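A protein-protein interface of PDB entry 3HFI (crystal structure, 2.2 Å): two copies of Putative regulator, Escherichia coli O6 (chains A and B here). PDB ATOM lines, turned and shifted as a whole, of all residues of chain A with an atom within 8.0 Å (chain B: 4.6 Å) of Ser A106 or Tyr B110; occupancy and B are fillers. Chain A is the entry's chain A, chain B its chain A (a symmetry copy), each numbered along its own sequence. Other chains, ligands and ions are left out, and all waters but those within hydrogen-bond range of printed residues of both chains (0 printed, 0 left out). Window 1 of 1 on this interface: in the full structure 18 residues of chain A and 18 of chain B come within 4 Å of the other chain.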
ATOM      1  N   PHE A  92      -7.466 -22.688   0.191  1.00  0.00           N
ATOM      2  CA  PHE A  92      -7.040 -23.847  -0.555  1.00  0.00           C
ATOM      3  C   PHE A  92      -7.417 -25.200   0.073  1.00  0.00           C
ATOM      4  O   PHE A  92      -7.900 -26.086  -0.642  1.00  0.00           O
ATOM      5  CB  PHE A  92      -5.591 -23.704  -0.953  1.00  0.00           C
ATOM      6  CG  PHE A  92      -5.393 -22.612  -1.962  1.00  0.00           C
ATOM      7  CD1 PHE A  92      -5.720 -22.814  -3.301  1.00  0.00           C
ATOM      8  CD2 PHE A  92      -4.982 -21.351  -1.575  1.00  0.00           C
ATOM      9  CE1 PHE A  92      -5.596 -21.793  -4.241  1.00  0.00           C
ATOM     10  CE2 PHE A  92      -4.829 -20.321  -2.540  1.00  0.00           C
ATOM     11  CZ  PHE A  92      -5.141 -20.560  -3.861  1.00  0.00           C
ATOM     12  N   GLU A  96      -9.914 -28.008  -1.696  1.00  0.00           N
ATOM     13  CA  GLU A  96      -9.600 -29.431  -1.688  1.00  0.00           C
ATOM     14  C   GLU A  96     -10.715 -30.247  -1.083  1.00  0.00           C
ATOM     15  O   GLU A  96     -11.107 -31.215  -1.703  1.00  0.00           O
ATOM     16  CB  GLU A  96      -8.247 -29.719  -0.996  1.00  0.00           C
ATOM     17  CG  GLU A  96      -7.029 -29.267  -1.815  1.00  0.00           C
ATOM     18  CD  GLU A  96      -5.737 -29.805  -1.269  1.00  0.00           C
ATOM     19  OE1 GLU A  96      -5.705 -30.073  -0.056  1.00  0.00           O
ATOM     20  OE2 GLU A  96      -4.763 -30.042  -2.023  1.00  0.00           O
ATOM     21  N   LYS A 102      -6.910 -33.173  -4.878  1.00  0.00           N
ATOM     22  CA  LYS A 102      -5.716 -32.559  -4.350  1.00  0.00           C
ATOM     23  C   LYS A 102      -5.179 -31.588  -5.373  1.00  0.00           C
ATOM     24  O   LYS A 102      -5.241 -31.831  -6.559  1.00  0.00           O
ATOM     25  CB  LYS A 102      -4.646 -33.629  -3.979  1.00  0.00           C
ATOM     26  CG  LYS A 102      -5.053 -34.455  -2.720  1.00  0.00           C
ATOM     27  CD  LYS A 102      -4.693 -35.953  -2.761  1.00  0.00           C
ATOM     28  CE  LYS A 102      -5.850 -36.884  -2.153  1.00  0.00           C
ATOM     29  NZ  LYS A 102      -5.653 -38.450  -2.094  1.00  0.00           N
ATOM     30  N   ILE A 103      -4.645 -30.476  -4.887  1.00  0.00           N
ATOM     31  CA  ILE A 103      -3.802 -29.573  -5.666  1.00  0.00           C
ATOM     32  C   ILE A 103      -2.425 -30.149  -5.900  1.00  0.00           C
ATOM     33  O   ILE A 103      -1.715 -30.468  -4.961  1.00  0.00           O
ATOM     34  CB  ILE A 103      -3.726 -28.198  -4.979  1.00  0.00           C
ATOM     35  CG1 ILE A 103      -5.143 -27.567  -5.016  1.00  0.00           C
ATOM     36  CG2 ILE A 103      -2.664 -27.295  -5.652  1.00  0.00           C
ATOM     37  CD1 ILE A 103      -5.246 -26.343  -4.170  1.00  0.00           C
ATOM     38  N   ARG A 104      -2.076 -30.327  -7.172  1.00  0.00           N
ATOM     39  CA  ARG A 104      -0.879 -30.952  -7.580  1.00  0.00           C
ATOM     40  C   ARG A 104       0.138 -30.112  -8.317  1.00  0.00           C
ATOM     41  O   ARG A 104       1.293 -30.544  -8.364  1.00  0.00           O
ATOM     42  CB  ARG A 104      -1.186 -32.158  -8.451  1.00  0.00           C
ATOM     43  CG  ARG A 104      -2.131 -33.154  -7.757  1.00  0.00           C
ATOM     44  CD  ARG A 104      -2.256 -34.411  -8.577  1.00  0.00           C
ATOM     45  NE  ARG A 104      -3.305 -35.238  -8.013  1.00  0.00           N
ATOM     46  CZ  ARG A 104      -3.117 -36.192  -7.125  1.00  0.00           C
ATOM     47  NH1 ARG A 104      -1.876 -36.502  -6.711  1.00  0.00           N
ATOM     48  NH2 ARG A 104      -4.182 -36.883  -6.671  1.00  0.00           N
ATOM     49  N   TYR A 105      -0.267 -28.969  -8.869  1.00  0.00           N
ATOM     50  CA  TYR A 105       0.627 -28.071  -9.589  1.00  0.00           C
ATOM     51  C   TYR A 105       0.241 -26.631  -9.459  1.00  0.00           C
ATOM     52  O   TYR A 105      -0.948 -26.278  -9.312  1.00  0.00           O
ATOM     53  CB  TYR A 105       0.693 -28.299 -11.116  1.00  0.00           C
ATOM     54  CG  TYR A 105       0.865 -29.721 -11.540  1.00  0.00           C
ATOM     55  CD1 TYR A 105       2.145 -30.218 -11.897  1.00  0.00           C
ATOM     56  CD2 TYR A 105      -0.222 -30.581 -11.628  1.00  0.00           C
ATOM     57  CE1 TYR A 105       2.319 -31.556 -12.293  1.00  0.00           C
ATOM     58  CE2 TYR A 105      -0.055 -31.905 -12.044  1.00  0.00           C
ATOM     59  CZ  TYR A 105       1.213 -32.378 -12.360  1.00  0.00           C
ATOM     60  OH  TYR A 105       1.382 -33.695 -12.745  1.00  0.00           O
ATOM     61  N   SER A 106       1.257 -25.815  -9.672  1.00  0.00           N
ATOM     62  CA  SER A 106       1.261 -24.371  -9.532  1.00  0.00           C
ATOM     63  C   SER A 106       2.199 -23.834 -10.606  1.00  0.00           C
ATOM     64  O   SER A 106       3.285 -24.393 -10.778  1.00  0.00           O
ATOM     65  CB  SER A 106       2.034 -24.038  -8.250  1.00  0.00           C
ATOM     66  OG  SER A 106       1.254 -23.195  -7.630  1.00  0.00           O
ATOM     67  N   GLU A 107       1.875 -22.678 -11.197  1.00  0.00           N
ATOM     68  CA  GLU A 107       2.812 -21.975 -12.040  1.00  0.00           C
ATOM     69  C   GLU A 107       2.702 -20.526 -11.594  1.00  0.00           C
ATOM     70  O   GLU A 107       1.606 -20.045 -11.426  1.00  0.00           O
ATOM     71  CB  GLU A 107       2.349 -22.016 -13.500  1.00  0.00           C
ATOM     72  CG  GLU A 107       2.449 -23.346 -14.156  1.00  0.00           C
ATOM     73  CD  GLU A 107       1.833 -23.383 -15.579  1.00  0.00           C
ATOM     74  OE1 GLU A 107       1.023 -22.507 -15.979  1.00  0.00           O
ATOM     75  OE2 GLU A 107       2.141 -24.353 -16.287  1.00  0.00           O
ATOM     76  N   SER A 108       3.811 -19.807 -11.507  1.00  0.00           N
ATOM     77  CA  SER A 108       3.744 -18.411 -11.237  1.00  0.00           C
ATOM     78  C   SER A 108       4.590 -17.665 -12.230  1.00  0.00           C
ATOM     79  O   SER A 108       5.614 -18.154 -12.679  1.00  0.00           O
ATOM     80  CB  SER A 108       4.301 -18.138  -9.839  1.00  0.00           C
ATOM     81  OG  SER A 108       3.667 -18.911  -8.860  1.00  0.00           O
ATOM     82  N   ARG A 109       4.235 -16.407 -12.425  1.00  0.00           N
ATOM     83  CA  ARG A 109       4.925 -15.500 -13.318  1.00  0.00           C
ATOM     84  C   ARG A 109       5.067 -14.206 -12.582  1.00  0.00           C
ATOM     85  O   ARG A 109       4.111 -13.754 -11.987  1.00  0.00           O
ATOM     86  CB  ARG A 109       4.066 -15.320 -14.536  1.00  0.00           C
ATOM     87  CG  ARG A 109       4.678 -14.523 -15.629  1.00  0.00           C
ATOM     88  CD  ARG A 109       3.690 -14.651 -16.778  1.00  0.00           C
ATOM     89  NE  ARG A 109       4.015 -13.855 -17.957  1.00  0.00           N
ATOM     90  CZ  ARG A 109       3.151 -13.627 -18.962  1.00  0.00           C
ATOM     91  NH1 ARG A 109       1.898 -14.136 -18.912  1.00  0.00           N
ATOM     92  NH2 ARG A 109       3.528 -12.874 -20.022  1.00  0.00           N
ATOM     93  N   GLU A 135       1.337 -13.501 -11.016  1.00  0.00           N
ATOM     94  CA  GLU A 135       0.142 -14.254 -11.458  1.00  0.00           C
ATOM     95  C   GLU A 135       0.427 -15.702 -11.172  1.00  0.00           C
ATOM     96  O   GLU A 135       1.460 -16.195 -11.572  1.00  0.00           O
ATOM     97  CB  GLU A 135      -0.104 -14.171 -12.960  1.00  0.00           C
ATOM     98  CG  GLU A 135      -0.494 -12.857 -13.506  1.00  0.00           C
ATOM     99  CD  GLU A 135      -0.687 -12.927 -15.036  1.00  0.00           C
ATOM    100  OE1 GLU A 135       0.052 -13.648 -15.721  1.00  0.00           O
ATOM    101  OE2 GLU A 135      -1.571 -12.296 -15.564  1.00  0.00           O
ATOM    102  N   GLN A 136      -0.513 -16.408 -10.571  1.00  0.00           N
ATOM    103  CA  GLN A 136      -0.316 -17.784 -10.228  1.00  0.00           C
ATOM    104  C   GLN A 136      -1.505 -18.600 -10.661  1.00  0.00           C
ATOM    105  O   GLN A 136      -2.657 -18.250 -10.363  1.00  0.00           O
ATOM    106  CB  GLN A 136      -0.199 -17.907  -8.725  1.00  0.00           C
ATOM    107  CG  GLN A 136       0.074 -19.357  -8.290  1.00  0.00           C
ATOM    108  CD  GLN A 136       0.180 -19.500  -6.822  1.00  0.00           C
ATOM    109  OE1 GLN A 136      -0.810 -19.244  -6.077  1.00  0.00           O
ATOM    110  NE2 GLN A 136       1.394 -19.895  -6.347  1.00  0.00           N
ATOM    111  N   LEU A 137      -1.241 -19.692 -11.338  1.00  0.00           N
ATOM    112  CA  LEU A 137      -2.280 -20.592 -11.790  1.00  0.00           C
ATOM    113  C   LEU A 137      -2.091 -21.863 -10.971  1.00  0.00           C
ATOM    114  O   LEU A 137      -1.022 -22.390 -10.937  1.00  0.00           O
ATOM    115  CB  LEU A 137      -2.138 -20.847 -13.304  1.00  0.00           C
ATOM    116  CG  LEU A 137      -3.278 -21.545 -14.041  1.00  0.00           C
ATOM    117  CD1 LEU A 137      -4.628 -20.906 -13.776  1.00  0.00           C
ATOM    118  CD2 LEU A 137      -3.020 -21.636 -15.548  1.00  0.00           C
ATOM    119  N   VAL A 138      -3.169 -22.341 -10.365  1.00  0.00           N
ATOM    120  CA  VAL A 138      -3.202 -23.496  -9.463  1.00  0.00           C
ATOM    121  C   VAL A 138      -4.081 -24.580 -10.081  1.00  0.00           C
ATOM    122  O   VAL A 138      -5.160 -24.278 -10.583  1.00  0.00           O
ATOM    123  CB  VAL A 138      -3.719 -23.065  -8.059  1.00  0.00           C
ATOM    124  CG1 VAL A 138      -3.790 -24.274  -7.096  1.00  0.00           C
ATOM    125  CG2 VAL A 138      -2.780 -21.953  -7.466  1.00  0.00           C
ATOM    126  N   PHE A 139      -3.589 -25.836 -10.082  1.00  0.00           N
ATOM    127  CA  PHE A 139      -4.172 -26.946 -10.828  1.00  0.00           C
ATOM    128  C   PHE A 139      -4.429 -28.109  -9.894  1.00  0.00           C
ATOM    129  O   PHE A 139      -3.609 -28.402  -9.004  1.00  0.00           O
ATOM    130  CB  PHE A 139      -3.211 -27.509 -11.851  1.00  0.00           C
ATOM    131  CG  PHE A 139      -2.830 -26.581 -12.970  1.00  0.00           C
ATOM    132  CD1 PHE A 139      -3.271 -26.816 -14.252  1.00  0.00           C
ATOM    133  CD2 PHE A 139      -1.926 -25.562 -12.758  1.00  0.00           C
ATOM    134  CE1 PHE A 139      -2.843 -26.003 -15.315  1.00  0.00           C
ATOM    135  CE2 PHE A 139      -1.481 -24.731 -13.789  1.00  0.00           C
ATOM    136  CZ  PHE A 139      -1.945 -24.963 -15.088  1.00  0.00           C
ATOM    137  N   PHE A 140      -5.536 -28.813 -10.134  1.00  0.00           N
ATOM    138  CA  PHE A 140      -5.703 -30.149  -9.617  1.00  0.00           C
ATOM    139  C   PHE A 140      -4.925 -31.175 -10.416  1.00  0.00           C
ATOM    140  O   PHE A 140      -4.332 -32.093  -9.889  1.00  0.00           O
ATOM    141  CB  PHE A 140      -7.168 -30.516  -9.706  1.00  0.00           C
ATOM    142  CG  PHE A 140      -8.053 -29.787  -8.737  1.00  0.00           C
ATOM    143  CD1 PHE A 140      -7.695 -29.632  -7.396  1.00  0.00           C
ATOM    144  CD2 PHE A 140      -9.271 -29.284  -9.164  1.00  0.00           C
ATOM    145  CE1 PHE A 140      -8.556 -28.981  -6.515  1.00  0.00           C
ATOM    146  CE2 PHE A 140     -10.162 -28.661  -8.263  1.00  0.00           C
ATOM    147  CZ  PHE A 140      -9.802 -28.513  -6.959  1.00  0.00           C
ATOM    148  N   SER A 141      -4.978 -31.080 -11.717  1.00  0.00           N
ATOM    149  CA  SER A 141      -4.244 -31.998 -12.532  1.00  0.00           C
ATOM    150  C   SER A 141      -3.688 -31.149 -13.623  1.00  0.00           C
ATOM    151  O   SER A 141      -4.106 -29.995 -13.797  1.00  0.00           O
ATOM    152  CB  SER A 141      -5.123 -33.101 -13.128  1.00  0.00           C
ATOM    153  OG  SER A 141      -6.031 -32.569 -14.095  1.00  0.00           O
ATOM    154  N   GLU A 147      -7.823 -22.388 -10.025  1.00  0.00           N
ATOM    155  CA  GLU A 147      -7.761 -21.039  -9.466  1.00  0.00           C
ATOM    156  C   GLU A 147      -6.672 -20.264 -10.129  1.00  0.00           C
ATOM    157  O   GLU A 147      -5.638 -20.850 -10.476  1.00  0.00           O
ATOM    158  CB  GLU A 147      -7.540 -21.081  -7.947  1.00  0.00           C
ATOM    159  CG  GLU A 147      -7.646 -19.730  -7.214  1.00  0.00           C
ATOM    160  CD  GLU A 147      -6.350 -18.951  -7.158  1.00  0.00           C
ATOM    161  OE1 GLU A 147      -5.264 -19.577  -7.089  1.00  0.00           O
ATOM    162  OE2 GLU A 147      -6.392 -17.710  -7.140  1.00  0.00           O
ATOM    163  N   TYR A 159       7.908 -17.002  -3.135  1.00  0.00           N
ATOM    164  CA  TYR A 159       7.242 -18.195  -3.577  1.00  0.00           C
ATOM    165  C   TYR A 159       8.357 -19.145  -3.962  1.00  0.00           C
ATOM    166  O   TYR A 159       8.126 -20.278  -4.279  1.00  0.00           O
ATOM    167  CB  TYR A 159       6.342 -17.894  -4.767  1.00  0.00           C
ATOM    168  N   SER B 106       8.186 -19.715 -12.212  1.00  0.00           N
ATOM    169  CA  SER B 106       8.257 -20.776 -11.226  1.00  0.00           C
ATOM    170  C   SER B 106       7.220 -21.816 -11.630  1.00  0.00           C
ATOM    171  O   SER B 106       6.099 -21.431 -11.974  1.00  0.00           O
ATOM    172  CB  SER B 106       7.658 -20.231  -9.922  1.00  0.00           C
ATOM    173  OG  SER B 106       8.542 -20.555  -9.018  1.00  0.00           O
ATOM    174  N   GLU B 107       7.516 -23.104 -11.432  1.00  0.00           N
ATOM    175  CA  GLU B 107       6.516 -24.136 -11.555  1.00  0.00           C
ATOM    176  C   GLU B 107       6.737 -25.020 -10.339  1.00  0.00           C
ATOM    177  O   GLU B 107       7.864 -25.346 -10.047  1.00  0.00           O
ATOM    178  CB  GLU B 107       6.797 -25.009 -12.783  1.00  0.00           C
ATOM    179  CG  GLU B 107       6.565 -24.346 -14.094  1.00  0.00           C
ATOM    180  CD  GLU B 107       7.002 -25.206 -15.309  1.00  0.00           C
ATOM    181  OE1 GLU B 107       7.794 -26.177 -15.189  1.00  0.00           O
ATOM    182  OE2 GLU B 107       6.572 -24.853 -16.416  1.00  0.00           O
ATOM    183  N   SER B 108       5.678 -25.493  -9.701  1.00  0.00           N
ATOM    184  CA  SER B 108       5.833 -26.440  -8.649  1.00  0.00           C
ATOM    185  C   SER B 108       4.905 -27.600  -8.876  1.00  0.00           C
ATOM    186  O   SER B 108       3.815 -27.442  -9.402  1.00  0.00           O
ATOM    187  CB  SER B 108       5.461 -25.786  -7.319  1.00  0.00           C
ATOM    188  OG  SER B 108       6.176 -24.604  -7.094  1.00  0.00           O
ATOM    189  N   ARG B 109       5.285 -28.732  -8.308  1.00  0.00           N
ATOM    190  CA  ARG B 109       4.529 -29.965  -8.377  1.00  0.00           C
ATOM    191  C   ARG B 109       4.531 -30.540  -6.996  1.00  0.00           C
ATOM    192  O   ARG B 109       5.570 -30.577  -6.370  1.00  0.00           O
ATOM    193  CB  ARG B 109       5.244 -30.882  -9.328  1.00  0.00           C
ATOM    194  CG  ARG B 109       4.537 -32.153  -9.630  1.00  0.00           C
ATOM    195  CD  ARG B 109       5.373 -32.789 -10.729  1.00  0.00           C
ATOM    196  NE  ARG B 109       4.941 -34.123 -11.134  1.00  0.00           N
ATOM    197  CZ  ARG B 109       5.687 -34.949 -11.888  1.00  0.00           C
ATOM    198  NH1 ARG B 109       6.915 -34.566 -12.309  1.00  0.00           N
ATOM    199  NH2 ARG B 109       5.216 -36.174 -12.220  1.00  0.00           N
ATOM    200  N   TYR B 110       3.367 -30.846  -6.478  1.00  0.00           N
ATOM    201  CA  TYR B 110       3.226 -31.229  -5.103  1.00  0.00           C
ATOM    202  C   TYR B 110       2.872 -32.734  -5.010  1.00  0.00           C
ATOM    203  O   TYR B 110       2.002 -33.207  -5.732  1.00  0.00           O
ATOM    204  CB  TYR B 110       2.122 -30.403  -4.424  1.00  0.00           C
ATOM    205  CG  TYR B 110       2.269 -28.896  -4.555  1.00  0.00           C
ATOM    206  CD1 TYR B 110       2.918 -28.134  -3.581  1.00  0.00           C
ATOM    207  CD2 TYR B 110       1.762 -28.230  -5.661  1.00  0.00           C
ATOM    208  CE1 TYR B 110       3.056 -26.721  -3.724  1.00  0.00           C
ATOM    209  CE2 TYR B 110       1.872 -26.830  -5.797  1.00  0.00           C
ATOM    210  CZ  TYR B 110       2.541 -26.088  -4.845  1.00  0.00           C
ATOM    211  OH  TYR B 110       2.643 -24.725  -5.021  1.00  0.00           O
ATOM    212  N   ALA B 111       3.483 -33.437  -4.068  1.00  0.00           N
ATOM    213  CA  ALA B 111       3.313 -34.896  -3.924  1.00  0.00           C
ATOM    214  C   ALA B 111       3.452 -35.313  -2.453  1.00  0.00           C
ATOM    215  O   ALA B 111       4.181 -34.686  -1.704  1.00  0.00           O
ATOM    216  CB  ALA B 111       4.360 -35.623  -4.777  1.00  0.00           C
ATOM    217  N   LEU B 132       4.720 -33.352   2.932  1.00  0.00           N
ATOM    218  CA  LEU B 132       4.453 -32.777   1.628  1.00  0.00           C
ATOM    219  C   LEU B 132       5.788 -32.581   0.933  1.00  0.00           C
ATOM    220  O   LEU B 132       6.726 -31.970   1.462  1.00  0.00           O
ATOM    221  CB  LEU B 132       3.674 -31.457   1.708  1.00  0.00           C
ATOM    222  CG  LEU B 132       3.413 -30.820   0.322  1.00  0.00           C
ATOM    223  CD1 LEU B 132       2.205 -31.506  -0.382  1.00  0.00           C
ATOM    224  CD2 LEU B 132       3.175 -29.322   0.437  1.00  0.00           C
ATOM    225  N   HIS B 133       5.870 -33.122  -0.268  1.00  0.00           N
ATOM    226  CA  HIS B 133       7.047 -32.941  -1.079  1.00  0.00           C
ATOM    227  C   HIS B 133       6.683 -32.016  -2.252  1.00  0.00           C
ATOM    228  O   HIS B 133       5.681 -32.217  -2.927  1.00  0.00           O
ATOM    229  CB  HIS B 133       7.546 -34.270  -1.593  1.00  0.00           C
ATOM    230  CG  HIS B 133       8.658 -34.151  -2.570  1.00  0.00           C
ATOM    231  ND1 HIS B 133       9.905 -33.670  -2.217  1.00  0.00           N
ATOM    232  CD2 HIS B 133       8.750 -34.511  -3.866  1.00  0.00           C
ATOM    233  CE1 HIS B 133      10.700 -33.689  -3.264  1.00  0.00           C
ATOM    234  NE2 HIS B 133      10.033 -34.204  -4.278  1.00  0.00           N
ATOM    235  N   LEU B 134       7.520 -31.030  -2.475  1.00  0.00           N
ATOM    236  CA  LEU B 134       7.397 -30.125  -3.598  1.00  0.00           C
ATOM    237  C   LEU B 134       8.633 -30.211  -4.464  1.00  0.00           C
ATOM    238  O   LEU B 134       9.758 -30.261  -3.940  1.00  0.00           O
ATOM    239  CB  LEU B 134       7.272 -28.760  -3.012  1.00  0.00           C
ATOM    240  CG  LEU B 134       7.082 -27.557  -3.854  1.00  0.00           C
ATOM    241  CD1 LEU B 134       5.763 -27.071  -3.309  1.00  0.00           C
ATOM    242  CD2 LEU B 134       8.183 -26.540  -3.598  1.00  0.00           C
ATOM    243  N   TYR B 159       2.737 -22.473  -0.927  1.00  0.00           N
ATOM    244  CA  TYR B 159       3.295 -21.821  -2.079  1.00  0.00           C
ATOM    245  C   TYR B 159       2.104 -21.254  -2.823  1.00  0.00           C
ATOM    246  O   TYR B 159       2.248 -20.557  -3.788  1.00  0.00           O
ATOM    247  CB  TYR B 159       4.057 -22.819  -2.940  1.00  0.00           C
ATOM    248  N   LEU B 160       0.911 -21.559  -2.351  1.00  0.00           N
ATOM    249  CA  LEU B 160      -0.277 -21.070  -3.008  1.00  0.00           C
ATOM    250  C   LEU B 160      -0.819 -19.845  -2.358  1.00  0.00           C
ATOM    251  O   LEU B 160      -0.866 -19.761  -1.174  1.00  0.00           O
ATOM    252  CB  LEU B 160      -1.347 -22.120  -2.980  1.00  0.00           C
ATOM    253  CG  LEU B 160      -0.823 -23.453  -3.391  1.00  0.00           C
ATOM    254  CD1 LEU B 160      -1.925 -24.369  -3.303  1.00  0.00           C
ATOM    255  CD2 LEU B 160      -0.389 -23.357  -4.758  1.00  0.00           C
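Ser A106 touches Glu B107, and with the chains exchanged Glu A107 touches Ser B106.
Ser A106 touches Ser B108, and with the chains exchanged Ser A108 touches Ser B106.
5 positions are printed for both chains.
Of the 17 pairs that touch across the chains among the printed residues, 4 have their exchanged pair printed and touching as well.
Of the 11 printed residues of chain B, 7 touch a printed residue of chain A.
Printed residues of chain B that touch a printed residue of chain A: Ser B106, Glu B107, Ser B108, Arg B109, Tyr B110, Tyr B159 and Leu B160.
Hydrophobic or aromatic side chains of chain B that line the printed part of chain A: Tyr B110 and Leu B160.
Among the printed residues, 17 pairs touch across the chains.
Among the printed residues, no Asp or Glu carboxylate lies within 4 Å of a Lys or Arg side-chain nitrogen of the other chain.
Of the printed residues of chain B, Ile A103 touches Tyr B110 (3.9 Å) and Leu B160 (3.8 Å).
Of the printed residues of chain B, Tyr A105 touches Ser B108 (3.3 Å), Arg B109 (3.5 Å) and Tyr B110 (3.9 Å).
Printed residues of chain B within 4 Å of Ser A106: Glu B107 (3.3 Å), Ser B108 (2.8 Å), Tyr B110 (3.3 Å) and Leu B160 (3.3 Å).
Of the printed residues of chain B, Glu A107 touches Ser B106.
Of the printed residues of chain B, Ser A108 touches Ser B106.
Of the printed residues of chain A, Arg B109 touches Arg A104 and Tyr A105.
Of chain A, only Ile A103 (3.9 Å), Arg A104 (2.8 Å), Tyr A105 (3.9 Å) and Ser A106 (3.3 Å) come within 4 Å of Tyr B110.
Leu B132 touches none of the printed residues of chain A.
The nearest residue of chain B that does not touch Ser A106 is Ser B106 (4.3 Å).
The nearest residue of chain A that does not touch Tyr B110 is Gln A136 (5.2 Å).
The nearest printed residue of chain B that does not touch Arg A104 is Ser B108 (4.1 Å).
O of Ile A103 touches CB of Tyr B110 (3.9 Å).
Leu B160 touches Ile A103 (CD1 to CG2, 3.8 Å).
Arg B109 touches Arg A104.
CA of Tyr A105 touches O of Ser B108, 3.3 Å away.
CG of Arg B109 touches CE1 of Tyr A105, 3.5 Å away.
Tyr A105 touches Tyr B110.
Ser A106 touches Glu B107.
CA of Glu A107 touches O of Ser B106, at 3.3 Å.
OE1 of Gln A136 touches CA of Leu B160 (3.6 Å).
Val A138 touches Leu B160 (CG2 to CD2, 3.9 Å).
The backbone NH of Arg A104 is in hydrogen-bond range of the backbone carbonyl oxygen of Phe A139 (3.1 Å).
N of Val A138 sits at hydrogen-bond distance from O of Glu A147 (2.9 Å).
The backbone carbonyl oxygen (O) of Tyr A105 is in hydrogen-bond range of the backbone NH (N) of Phe A139 (2.8 Å).
The side-chain carboxylate (OE2) of Glu A96 is in hydrogen-bond range of the backbone NH (N) of Ile A103.
The backbone NH (N) of Leu A137 sits at hydrogen-bond distance from the backbone carbonyl oxygen (O) of Glu A107 (2.9 Å).
The backbone NH (N) of Ser B108 lies within hydrogen-bond range of the backbone carbonyl oxygen (O) of Ser A106 (2.8 Å).
The backbone carbonyl oxygen of Arg A104 sits at hydrogen-bond distance from the backbone NH of Tyr B110 (2.8 Å).
NE2 of Gln A136 is in hydrogen-bond range of O of Tyr B159, at 2.8 Å.
The backbone carbonyl oxygen (O) of Ser B106 sits at hydrogen-bond distance from the backbone NH (N) of Ser A108, 2.8 Å away.
OH of Tyr B110 lies within hydrogen-bond range of OG of Ser A106 (3.3 Å).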
